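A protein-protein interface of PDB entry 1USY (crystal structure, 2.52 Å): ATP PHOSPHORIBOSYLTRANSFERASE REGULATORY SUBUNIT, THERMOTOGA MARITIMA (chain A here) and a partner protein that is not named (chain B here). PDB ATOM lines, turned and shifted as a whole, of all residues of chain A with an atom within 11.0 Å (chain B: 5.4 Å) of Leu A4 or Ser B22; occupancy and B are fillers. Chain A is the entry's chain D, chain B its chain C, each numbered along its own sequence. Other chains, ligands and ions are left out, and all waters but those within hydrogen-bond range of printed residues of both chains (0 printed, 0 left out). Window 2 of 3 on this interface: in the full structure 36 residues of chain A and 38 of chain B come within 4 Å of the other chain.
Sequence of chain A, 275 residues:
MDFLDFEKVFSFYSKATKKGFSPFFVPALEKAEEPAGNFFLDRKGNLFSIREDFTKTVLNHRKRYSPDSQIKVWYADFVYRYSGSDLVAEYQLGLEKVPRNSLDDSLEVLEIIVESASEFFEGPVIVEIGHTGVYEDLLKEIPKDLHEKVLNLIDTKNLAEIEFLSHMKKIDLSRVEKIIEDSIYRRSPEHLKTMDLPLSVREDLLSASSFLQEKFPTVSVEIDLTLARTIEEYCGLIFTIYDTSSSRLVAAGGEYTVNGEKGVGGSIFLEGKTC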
ATOM      1  N   ASP A   2     -26.339 -25.691  -9.527  1.00  0.00           N
ATOM      2  CA  ASP A   2     -25.800 -25.098 -10.784  1.00  0.00           C
ATOM      3  C   ASP A   2     -26.011 -23.575 -10.894  1.00  0.00           C
ATOM      4  O   ASP A   2     -26.822 -23.101 -11.709  1.00  0.00           O
ATOM      5  CB  ASP A   2     -26.366 -25.806 -12.029  1.00  0.00           C
ATOM      6  CG  ASP A   2     -25.454 -25.666 -13.256  1.00  0.00           C
ATOM      7  OD1 ASP A   2     -25.794 -24.912 -14.193  1.00  0.00           O
ATOM      8  OD2 ASP A   2     -24.368 -26.280 -13.371  1.00  0.00           O
ATOM      9  N   PHE A   3     -25.285 -22.826 -10.061  1.00  0.00           N
ATOM     10  CA  PHE A   3     -25.084 -21.390 -10.259  1.00  0.00           C
ATOM     11  C   PHE A   3     -23.900 -21.346 -11.193  1.00  0.00           C
ATOM     12  O   PHE A   3     -22.842 -21.899 -10.862  1.00  0.00           O
ATOM     13  CB  PHE A   3     -24.731 -20.687  -8.945  1.00  0.00           C
ATOM     14  CG  PHE A   3     -25.474 -21.219  -7.754  1.00  0.00           C
ATOM     15  CD1 PHE A   3     -24.875 -22.135  -6.903  1.00  0.00           C
ATOM     16  CD2 PHE A   3     -26.776 -20.819  -7.498  1.00  0.00           C
ATOM     17  CE1 PHE A   3     -25.559 -22.645  -5.806  1.00  0.00           C
ATOM     18  CE2 PHE A   3     -27.469 -21.323  -6.400  1.00  0.00           C
ATOM     19  CZ  PHE A   3     -26.855 -22.240  -5.551  1.00  0.00           C
ATOM     20  N   LEU A   4     -24.075 -20.740 -12.360  1.00  0.00           N
ATOM     21  CA  LEU A   4     -23.074 -20.779 -13.439  1.00  0.00           C
ATOM     22  C   LEU A   4     -23.589 -19.918 -14.566  1.00  0.00           C
ATOM     23  O   LEU A   4     -22.843 -19.462 -15.435  1.00  0.00           O
ATOM     24  CB  LEU A   4     -22.867 -22.201 -13.951  1.00  0.00           C
ATOM     25  CG  LEU A   4     -21.474 -22.487 -14.534  1.00  0.00           C
ATOM     26  CD1 LEU A   4     -20.534 -23.177 -13.529  1.00  0.00           C
ATOM     27  CD2 LEU A   4     -21.578 -23.323 -15.808  1.00  0.00           C
ATOM     28  N   ASP A   5     -24.898 -19.736 -14.519  1.00  0.00           N
ATOM     29  CA  ASP A   5     -25.624 -18.826 -15.361  1.00  0.00           C
ATOM     30  C   ASP A   5     -25.182 -17.399 -15.032  1.00  0.00           C
ATOM     31  O   ASP A   5     -25.287 -16.494 -15.865  1.00  0.00           O
ATOM     32  CB  ASP A   5     -27.116 -18.984 -15.059  1.00  0.00           C
ATOM     33  CG  ASP A   5     -27.891 -19.560 -16.224  1.00  0.00           C
ATOM     34  OD1 ASP A   5     -29.109 -19.252 -16.334  1.00  0.00           O
ATOM     35  OD2 ASP A   5     -27.353 -20.308 -17.087  1.00  0.00           O
ATOM     36  N   PHE A   6     -24.669 -17.230 -13.813  1.00  0.00           N
ATOM     37  CA  PHE A   6     -24.322 -15.922 -13.278  1.00  0.00           C
ATOM     38  C   PHE A   6     -23.035 -15.354 -13.895  1.00  0.00           C
ATOM     39  O   PHE A   6     -22.600 -14.265 -13.518  1.00  0.00           O
ATOM     40  CB  PHE A   6     -24.235 -15.955 -11.732  1.00  0.00           C
ATOM     41  CG  PHE A   6     -25.554 -16.274 -11.041  1.00  0.00           C
ATOM     42  CD1 PHE A   6     -25.850 -17.568 -10.641  1.00  0.00           C
ATOM     43  CD2 PHE A   6     -26.475 -15.288 -10.790  1.00  0.00           C
ATOM     44  CE1 PHE A   6     -27.061 -17.884 -10.011  1.00  0.00           C
ATOM     45  CE2 PHE A   6     -27.687 -15.590 -10.150  1.00  0.00           C
ATOM     46  CZ  PHE A   6     -27.980 -16.894  -9.759  1.00  0.00           C
ATOM     47  N   GLU A   7     -22.433 -16.081 -14.835  1.00  0.00           N
ATOM     48  CA  GLU A   7     -21.298 -15.554 -15.582  1.00  0.00           C
ATOM     49  C   GLU A   7     -21.747 -14.570 -16.648  1.00  0.00           C
ATOM     50  O   GLU A   7     -20.983 -13.676 -17.004  1.00  0.00           O
ATOM     51  CB  GLU A   7     -20.548 -16.663 -16.285  1.00  0.00           C
ATOM     52  CG  GLU A   7     -20.062 -17.757 -15.366  1.00  0.00           C
ATOM     53  CD  GLU A   7     -19.195 -18.780 -16.071  1.00  0.00           C
ATOM     54  OE1 GLU A   7     -19.498 -19.186 -17.230  1.00  0.00           O
ATOM     55  OE2 GLU A   7     -18.211 -19.201 -15.449  1.00  0.00           O
ATOM     56  N   LYS A   8     -22.956 -14.760 -17.187  1.00  0.00           N
ATOM     57  CA  LYS A   8     -23.514 -13.867 -18.215  1.00  0.00           C
ATOM     58  C   LYS A   8     -23.532 -12.402 -17.746  1.00  0.00           C
ATOM     59  O   LYS A   8     -23.756 -11.478 -18.539  1.00  0.00           O
ATOM     60  CB  LYS A   8     -24.938 -14.301 -18.579  1.00  0.00           C
ATOM     61  CG  LYS A   8     -24.998 -15.685 -19.203  1.00  0.00           C
ATOM     62  CD  LYS A   8     -26.428 -16.217 -19.274  1.00  0.00           C
ATOM     63  CE  LYS A   8     -26.423 -17.551 -20.007  1.00  0.00           C
ATOM     64  NZ  LYS A   8     -27.721 -18.231 -19.994  1.00  0.00           N
ATOM     65  N   VAL A   9     -23.272 -12.222 -16.447  1.00  0.00           N
ATOM     66  CA  VAL A   9     -23.285 -10.934 -15.772  1.00  0.00           C
ATOM     67  C   VAL A   9     -22.105 -10.059 -16.202  1.00  0.00           C
ATOM     68  O   VAL A   9     -22.229  -8.825 -16.311  1.00  0.00           O
ATOM     69  CB  VAL A   9     -23.248 -11.153 -14.267  1.00  0.00           C
ATOM     70  CG1 VAL A   9     -23.289  -9.827 -13.514  1.00  0.00           C
ATOM     71  CG2 VAL A   9     -24.442 -11.990 -13.876  1.00  0.00           C
ATOM     72  N   PHE A  10     -20.974 -10.710 -16.460  1.00  0.00           N
ATOM     73  CA  PHE A  10     -19.755 -10.020 -16.846  1.00  0.00           C
ATOM     74  C   PHE A  10     -19.891  -9.596 -18.294  1.00  0.00           C
ATOM     75  O   PHE A  10     -19.455  -8.508 -18.681  1.00  0.00           O
ATOM     76  CB  PHE A  10     -18.505 -10.890 -16.543  1.00  0.00           C
ATOM     77  CG  PHE A  10     -18.321 -11.146 -15.068  1.00  0.00           C
ATOM     78  CD1 PHE A  10     -18.053 -10.088 -14.199  1.00  0.00           C
ATOM     79  CD2 PHE A  10     -18.495 -12.430 -14.526  1.00  0.00           C
ATOM     80  CE1 PHE A  10     -17.937 -10.308 -12.814  1.00  0.00           C
ATOM     81  CE2 PHE A  10     -18.381 -12.668 -13.126  1.00  0.00           C
ATOM     82  CZ  PHE A  10     -18.115 -11.603 -12.281  1.00  0.00           C
ATOM     83  N   SER A  11     -20.531 -10.453 -19.082  1.00  0.00           N
ATOM     84  CA  SER A  11     -20.902 -10.130 -20.450  1.00  0.00           C
ATOM     85  C   SER A  11     -21.837  -8.888 -20.439  1.00  0.00           C
ATOM     86  O   SER A  11     -21.610  -7.891 -21.173  1.00  0.00           O
ATOM     87  CB  SER A  11     -21.590 -11.334 -21.068  1.00  0.00           C
ATOM     88  OG  SER A  11     -21.820 -11.110 -22.428  1.00  0.00           O
ATOM     89  N   PHE A  78     -30.838  -9.899  -6.926  1.00  0.00           N
ATOM     90  CA  PHE A  78     -32.124 -10.475  -6.652  1.00  0.00           C
ATOM     91  C   PHE A  78     -33.201  -9.450  -6.452  1.00  0.00           C
ATOM     92  O   PHE A  78     -32.951  -8.404  -5.873  1.00  0.00           O
ATOM     93  CB  PHE A  78     -32.031 -11.383  -5.431  1.00  0.00           C
ATOM     94  CG  PHE A  78     -31.300 -12.595  -5.715  1.00  0.00           C
ATOM     95  CD1 PHE A  78     -29.949 -12.654  -5.455  1.00  0.00           C
ATOM     96  CD2 PHE A  78     -31.935 -13.654  -6.372  1.00  0.00           C
ATOM     97  CE1 PHE A  78     -29.229 -13.809  -5.762  1.00  0.00           C
ATOM     98  CE2 PHE A  78     -31.234 -14.813  -6.693  1.00  0.00           C
ATOM     99  CZ  PHE A  78     -29.872 -14.898  -6.377  1.00  0.00           C
ATOM    100  N   TYR A  91     -33.039 -13.643  -9.969  1.00  0.00           N
ATOM    101  CA  TYR A  91     -31.951 -12.752 -10.319  1.00  0.00           C
ATOM    102  C   TYR A  91     -32.336 -11.917 -11.518  1.00  0.00           C
ATOM    103  O   TYR A  91     -32.947 -12.447 -12.417  1.00  0.00           O
ATOM    104  CB  TYR A  91     -30.755 -13.584 -10.658  1.00  0.00           C
ATOM    105  CG  TYR A  91     -29.469 -12.831 -10.585  1.00  0.00           C
ATOM    106  CD1 TYR A  91     -28.850 -12.582  -9.352  1.00  0.00           C
ATOM    107  CD2 TYR A  91     -28.842 -12.410 -11.752  1.00  0.00           C
ATOM    108  CE1 TYR A  91     -27.642 -11.935  -9.301  1.00  0.00           C
ATOM    109  CE2 TYR A  91     -27.639 -11.757 -11.708  1.00  0.00           C
ATOM    110  CZ  TYR A  91     -27.038 -11.517 -10.481  1.00  0.00           C
ATOM    111  OH  TYR A  91     -25.837 -10.851 -10.446  1.00  0.00           O
ATOM    112  N   LEU A  93     -30.890  -8.723 -14.413  1.00  0.00           N
ATOM    113  CA  LEU A  93     -29.889  -7.826 -14.935  1.00  0.00           C
ATOM    114  C   LEU A  93     -30.693  -6.741 -15.608  1.00  0.00           C
ATOM    115  O   LEU A  93     -31.621  -7.037 -16.348  1.00  0.00           O
ATOM    116  CB  LEU A  93     -29.019  -8.500 -15.992  1.00  0.00           C
ATOM    117  CG  LEU A  93     -28.179  -9.734 -15.666  1.00  0.00           C
ATOM    118  CD1 LEU A  93     -27.819 -10.501 -16.943  1.00  0.00           C
ATOM    119  CD2 LEU A  93     -26.920  -9.262 -15.057  1.00  0.00           C
ATOM    120  N   PHE A 120     -28.077 -14.971 -24.264  1.00  0.00           N
ATOM    121  CA  PHE A 120     -28.282 -15.731 -23.019  1.00  0.00           C
ATOM    122  C   PHE A 120     -29.255 -16.895 -23.142  1.00  0.00           C
ATOM    123  O   PHE A 120     -29.298 -17.768 -22.276  1.00  0.00           O
ATOM    124  CB  PHE A 120     -28.765 -14.813 -21.863  1.00  0.00           C
ATOM    125  CG  PHE A 120     -27.805 -13.712 -21.497  1.00  0.00           C
ATOM    126  CD1 PHE A 120     -28.145 -12.793 -20.543  1.00  0.00           C
ATOM    127  CD2 PHE A 120     -26.548 -13.607 -22.099  1.00  0.00           C
ATOM    128  CE1 PHE A 120     -27.254 -11.771 -20.206  1.00  0.00           C
ATOM    129  CE2 PHE A 120     -25.683 -12.588 -21.769  1.00  0.00           C
ATOM    130  CZ  PHE A 120     -26.030 -11.683 -20.824  1.00  0.00           C
ATOM    131  N   LEU A 270     -32.858 -14.092 -15.662  1.00  0.00           N
ATOM    132  CA  LEU A 270     -32.134 -15.375 -15.990  1.00  0.00           C
ATOM    133  C   LEU A 270     -33.041 -16.554 -15.604  1.00  0.00           C
ATOM    134  O   LEU A 270     -33.028 -17.002 -14.447  1.00  0.00           O
ATOM    135  CB  LEU A 270     -30.863 -15.639 -15.166  1.00  0.00           C
ATOM    136  CG  LEU A 270     -29.699 -14.662 -15.184  1.00  0.00           C
ATOM    137  CD1 LEU A 270     -28.682 -15.085 -14.121  1.00  0.00           C
ATOM    138  CD2 LEU A 270     -28.930 -14.600 -16.515  1.00  0.00           C
ATOM    139  N   GLU A 271     -33.792 -17.043 -16.551  1.00  0.00           N
ATOM    140  CA  GLU A 271     -34.795 -18.099 -16.297  1.00  0.00           C
ATOM    141  C   GLU A 271     -36.095 -17.360 -15.991  1.00  0.00           C
ATOM    142  O   GLU A 271     -36.548 -16.555 -16.792  1.00  0.00           O
ATOM    143  CB  GLU A 271     -34.388 -18.958 -15.121  1.00  0.00           C
ATOM    144  N   THR B  17     -11.814 -18.258 -11.110  1.00  0.00           N
ATOM    145  CA  THR B  17     -12.132 -19.241 -12.142  1.00  0.00           C
ATOM    146  C   THR B  17     -10.856 -19.815 -12.746  1.00  0.00           C
ATOM    147  O   THR B  17     -10.887 -20.898 -13.334  1.00  0.00           O
ATOM    148  CB  THR B  17     -13.173 -18.743 -13.261  1.00  0.00           C
ATOM    149  OG1 THR B  17     -12.820 -17.454 -13.739  1.00  0.00           O
ATOM    150  CG2 THR B  17     -14.567 -18.493 -12.669  1.00  0.00           C
ATOM    151  N   GLY B  20     -10.564 -23.018 -10.965  1.00  0.00           N
ATOM    152  CA  GLY B  20     -11.696 -23.915 -10.841  1.00  0.00           C
ATOM    153  C   GLY B  20     -12.658 -23.591  -9.716  1.00  0.00           C
ATOM    154  O   GLY B  20     -13.387 -24.458  -9.218  1.00  0.00           O
ATOM    155  N   PHE B  21     -12.647 -22.333  -9.300  1.00  0.00           N
ATOM    156  CA  PHE B  21     -13.675 -21.853  -8.426  1.00  0.00           C
ATOM    157  C   PHE B  21     -14.845 -21.453  -9.322  1.00  0.00           C
ATOM    158  O   PHE B  21     -14.655 -20.790 -10.345  1.00  0.00           O
ATOM    159  CB  PHE B  21     -13.167 -20.714  -7.551  1.00  0.00           C
ATOM    160  CG  PHE B  21     -12.330 -21.182  -6.386  1.00  0.00           C
ATOM    161  CD1 PHE B  21     -10.976 -21.534  -6.565  1.00  0.00           C
ATOM    162  CD2 PHE B  21     -12.894 -21.297  -5.119  1.00  0.00           C
ATOM    163  CE1 PHE B  21     -10.192 -21.995  -5.484  1.00  0.00           C
ATOM    164  CE2 PHE B  21     -12.124 -21.715  -4.034  1.00  0.00           C
ATOM    165  CZ  PHE B  21     -10.750 -22.089  -4.236  1.00  0.00           C
ATOM    166  N   SER B  22     -16.035 -21.890  -8.927  1.00  0.00           N
ATOM    167  CA  SER B  22     -17.291 -21.705  -9.651  1.00  0.00           C
ATOM    168  C   SER B  22     -18.099 -20.631  -8.914  1.00  0.00           C
ATOM    169  O   SER B  22     -17.764 -20.282  -7.792  1.00  0.00           O
ATOM    170  CB  SER B  22     -18.082 -23.030  -9.636  1.00  0.00           C
ATOM    171  OG  SER B  22     -17.870 -23.751 -10.832  1.00  0.00           O
ATOM    172  N   PRO B  23     -19.148 -20.104  -9.535  1.00  0.00           N
ATOM    173  CA  PRO B  23     -19.974 -19.068  -8.913  1.00  0.00           C
ATOM    174  C   PRO B  23     -20.946 -19.568  -7.861  1.00  0.00           C
ATOM    175  O   PRO B  23     -21.273 -20.717  -7.834  1.00  0.00           O
ATOM    176  CB  PRO B  23     -20.754 -18.484 -10.087  1.00  0.00           C
ATOM    177  CG  PRO B  23     -20.222 -19.152 -11.316  1.00  0.00           C
ATOM    178  CD  PRO B  23     -19.594 -20.426 -10.899  1.00  0.00           C
ATOM    179  N   PHE B  24     -21.367 -18.677  -6.981  1.00  0.00           N
ATOM    180  CA  PHE B  24     -22.308 -18.986  -5.911  1.00  0.00           C
ATOM    181  C   PHE B  24     -23.129 -17.718  -5.569  1.00  0.00           C
ATOM    182  O   PHE B  24     -22.606 -16.770  -4.979  1.00  0.00           O
ATOM    183  CB  PHE B  24     -21.567 -19.530  -4.669  1.00  0.00           C
ATOM    184  CG  PHE B  24     -22.479 -19.836  -3.527  1.00  0.00           C
ATOM    185  CD1 PHE B  24     -23.219 -21.003  -3.505  1.00  0.00           C
ATOM    186  CD2 PHE B  24     -22.645 -18.935  -2.506  1.00  0.00           C
ATOM    187  CE1 PHE B  24     -24.083 -21.272  -2.451  1.00  0.00           C
ATOM    188  CE2 PHE B  24     -23.522 -19.193  -1.439  1.00  0.00           C
ATOM    189  CZ  PHE B  24     -24.233 -20.351  -1.410  1.00  0.00           C
ATOM    190  N   LYS B  72     -15.959 -25.966  -5.099  1.00  0.00           N
ATOM    191  CA  LYS B  72     -15.204 -24.735  -5.049  1.00  0.00           C
ATOM    192  C   LYS B  72     -16.270 -23.723  -5.213  1.00  0.00           C
ATOM    193  O   LYS B  72     -17.409 -24.097  -5.481  1.00  0.00           O
ATOM    194  CB  LYS B  72     -14.225 -24.668  -6.176  1.00  0.00           C
ATOM    195  CG  LYS B  72     -12.843 -24.984  -5.716  1.00  0.00           C
ATOM    196  CD  LYS B  72     -12.443 -26.328  -6.214  1.00  0.00           C
ATOM    197  CE  LYS B  72     -10.938 -26.464  -6.358  1.00  0.00           C
ATOM    198  NZ  LYS B  72     -10.178 -25.250  -6.700  1.00  0.00           N
ATOM    199  N   VAL B  73     -15.983 -22.474  -4.951  1.00  0.00           N
ATOM    200  CA  VAL B  73     -16.938 -21.419  -5.254  1.00  0.00           C
ATOM    201  C   VAL B  73     -16.330 -20.137  -4.865  1.00  0.00           C
ATOM    202  O   VAL B  73     -15.576 -20.090  -3.870  1.00  0.00           O
ATOM    203  CB  VAL B  73     -18.342 -21.558  -4.594  1.00  0.00           C
ATOM    204  CG1 VAL B  73     -19.133 -22.694  -5.209  1.00  0.00           C
ATOM    205  CG2 VAL B  73     -18.293 -21.695  -3.060  1.00  0.00           C
ATOM    206  N   TRP B  74     -16.649 -19.106  -5.653  1.00  0.00           N
ATOM    207  CA  TRP B  74     -16.417 -17.708  -5.268  1.00  0.00           C
ATOM    208  C   TRP B  74     -17.751 -17.026  -5.156  1.00  0.00           C
ATOM    209  O   TRP B  74     -18.726 -17.485  -5.775  1.00  0.00           O
ATOM    210  CB  TRP B  74     -15.552 -17.013  -6.324  1.00  0.00           C
ATOM    211  CG  TRP B  74     -16.226 -16.925  -7.645  1.00  0.00           C
ATOM    212  CD1 TRP B  74     -16.161 -17.824  -8.656  1.00  0.00           C
ATOM    213  CD2 TRP B  74     -17.054 -15.859  -8.107  1.00  0.00           C
ATOM    214  NE1 TRP B  74     -16.917 -17.399  -9.723  1.00  0.00           N
ATOM    215  CE2 TRP B  74     -17.467 -16.187  -9.418  1.00  0.00           C
ATOM    216  CE3 TRP B  74     -17.469 -14.645  -7.558  1.00  0.00           C
ATOM    217  CZ2 TRP B  74     -18.298 -15.368 -10.168  1.00  0.00           C
ATOM    218  CZ3 TRP B  74     -18.316 -13.842  -8.295  1.00  0.00           C
ATOM    219  CH2 TRP B  74     -18.715 -14.199  -9.592  1.00  0.00           C
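N of Phe B24 sits at hydrogen-bond distance from O of Trp B74, at 3.1 Å. The backbone NH (N) of Trp B74 is in hydrogen-bond range of the backbone carbonyl oxygen (O) of Ser B22 (2.7 Å).
Among the printed residues, merely in contact across the chains: Phe A3 with Pro B23, Phe A3 with Phe B24, Phe A10 with Trp B74, Leu A4 with Ser B22 and Leu A4 with Pro B23.
Of the printed residues of chain B, Phe A3 touches Pro B23 (3.6 Å) and Phe B24 (3.7 Å). Leu A4 touches just these residues of chain B: Ser B22 and Pro B23. Phe A6 touches none of the printed residues of chain B. Printed residues of chain B within 4 Å of Phe A10: Trp B74. Gly B20 touches none of the printed residues of chain A. Ser B22 touches one residue of chain A. Of the printed residues of chain A, Phe B24 touches Phe A3 (3.7 Å). No residue of chain A comes within 4 Å of Val B73. Of chain A, only Phe A10 comes within 4 Å of Trp B74. The nearest printed residue of chain A that does not touch Phe B24 is Phe A6 (5.8 Å).
Of the 9 printed residues of chain B, 4 touch a printed residue of chain A. Among the printed residues, 5 pairs touch across the chains.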
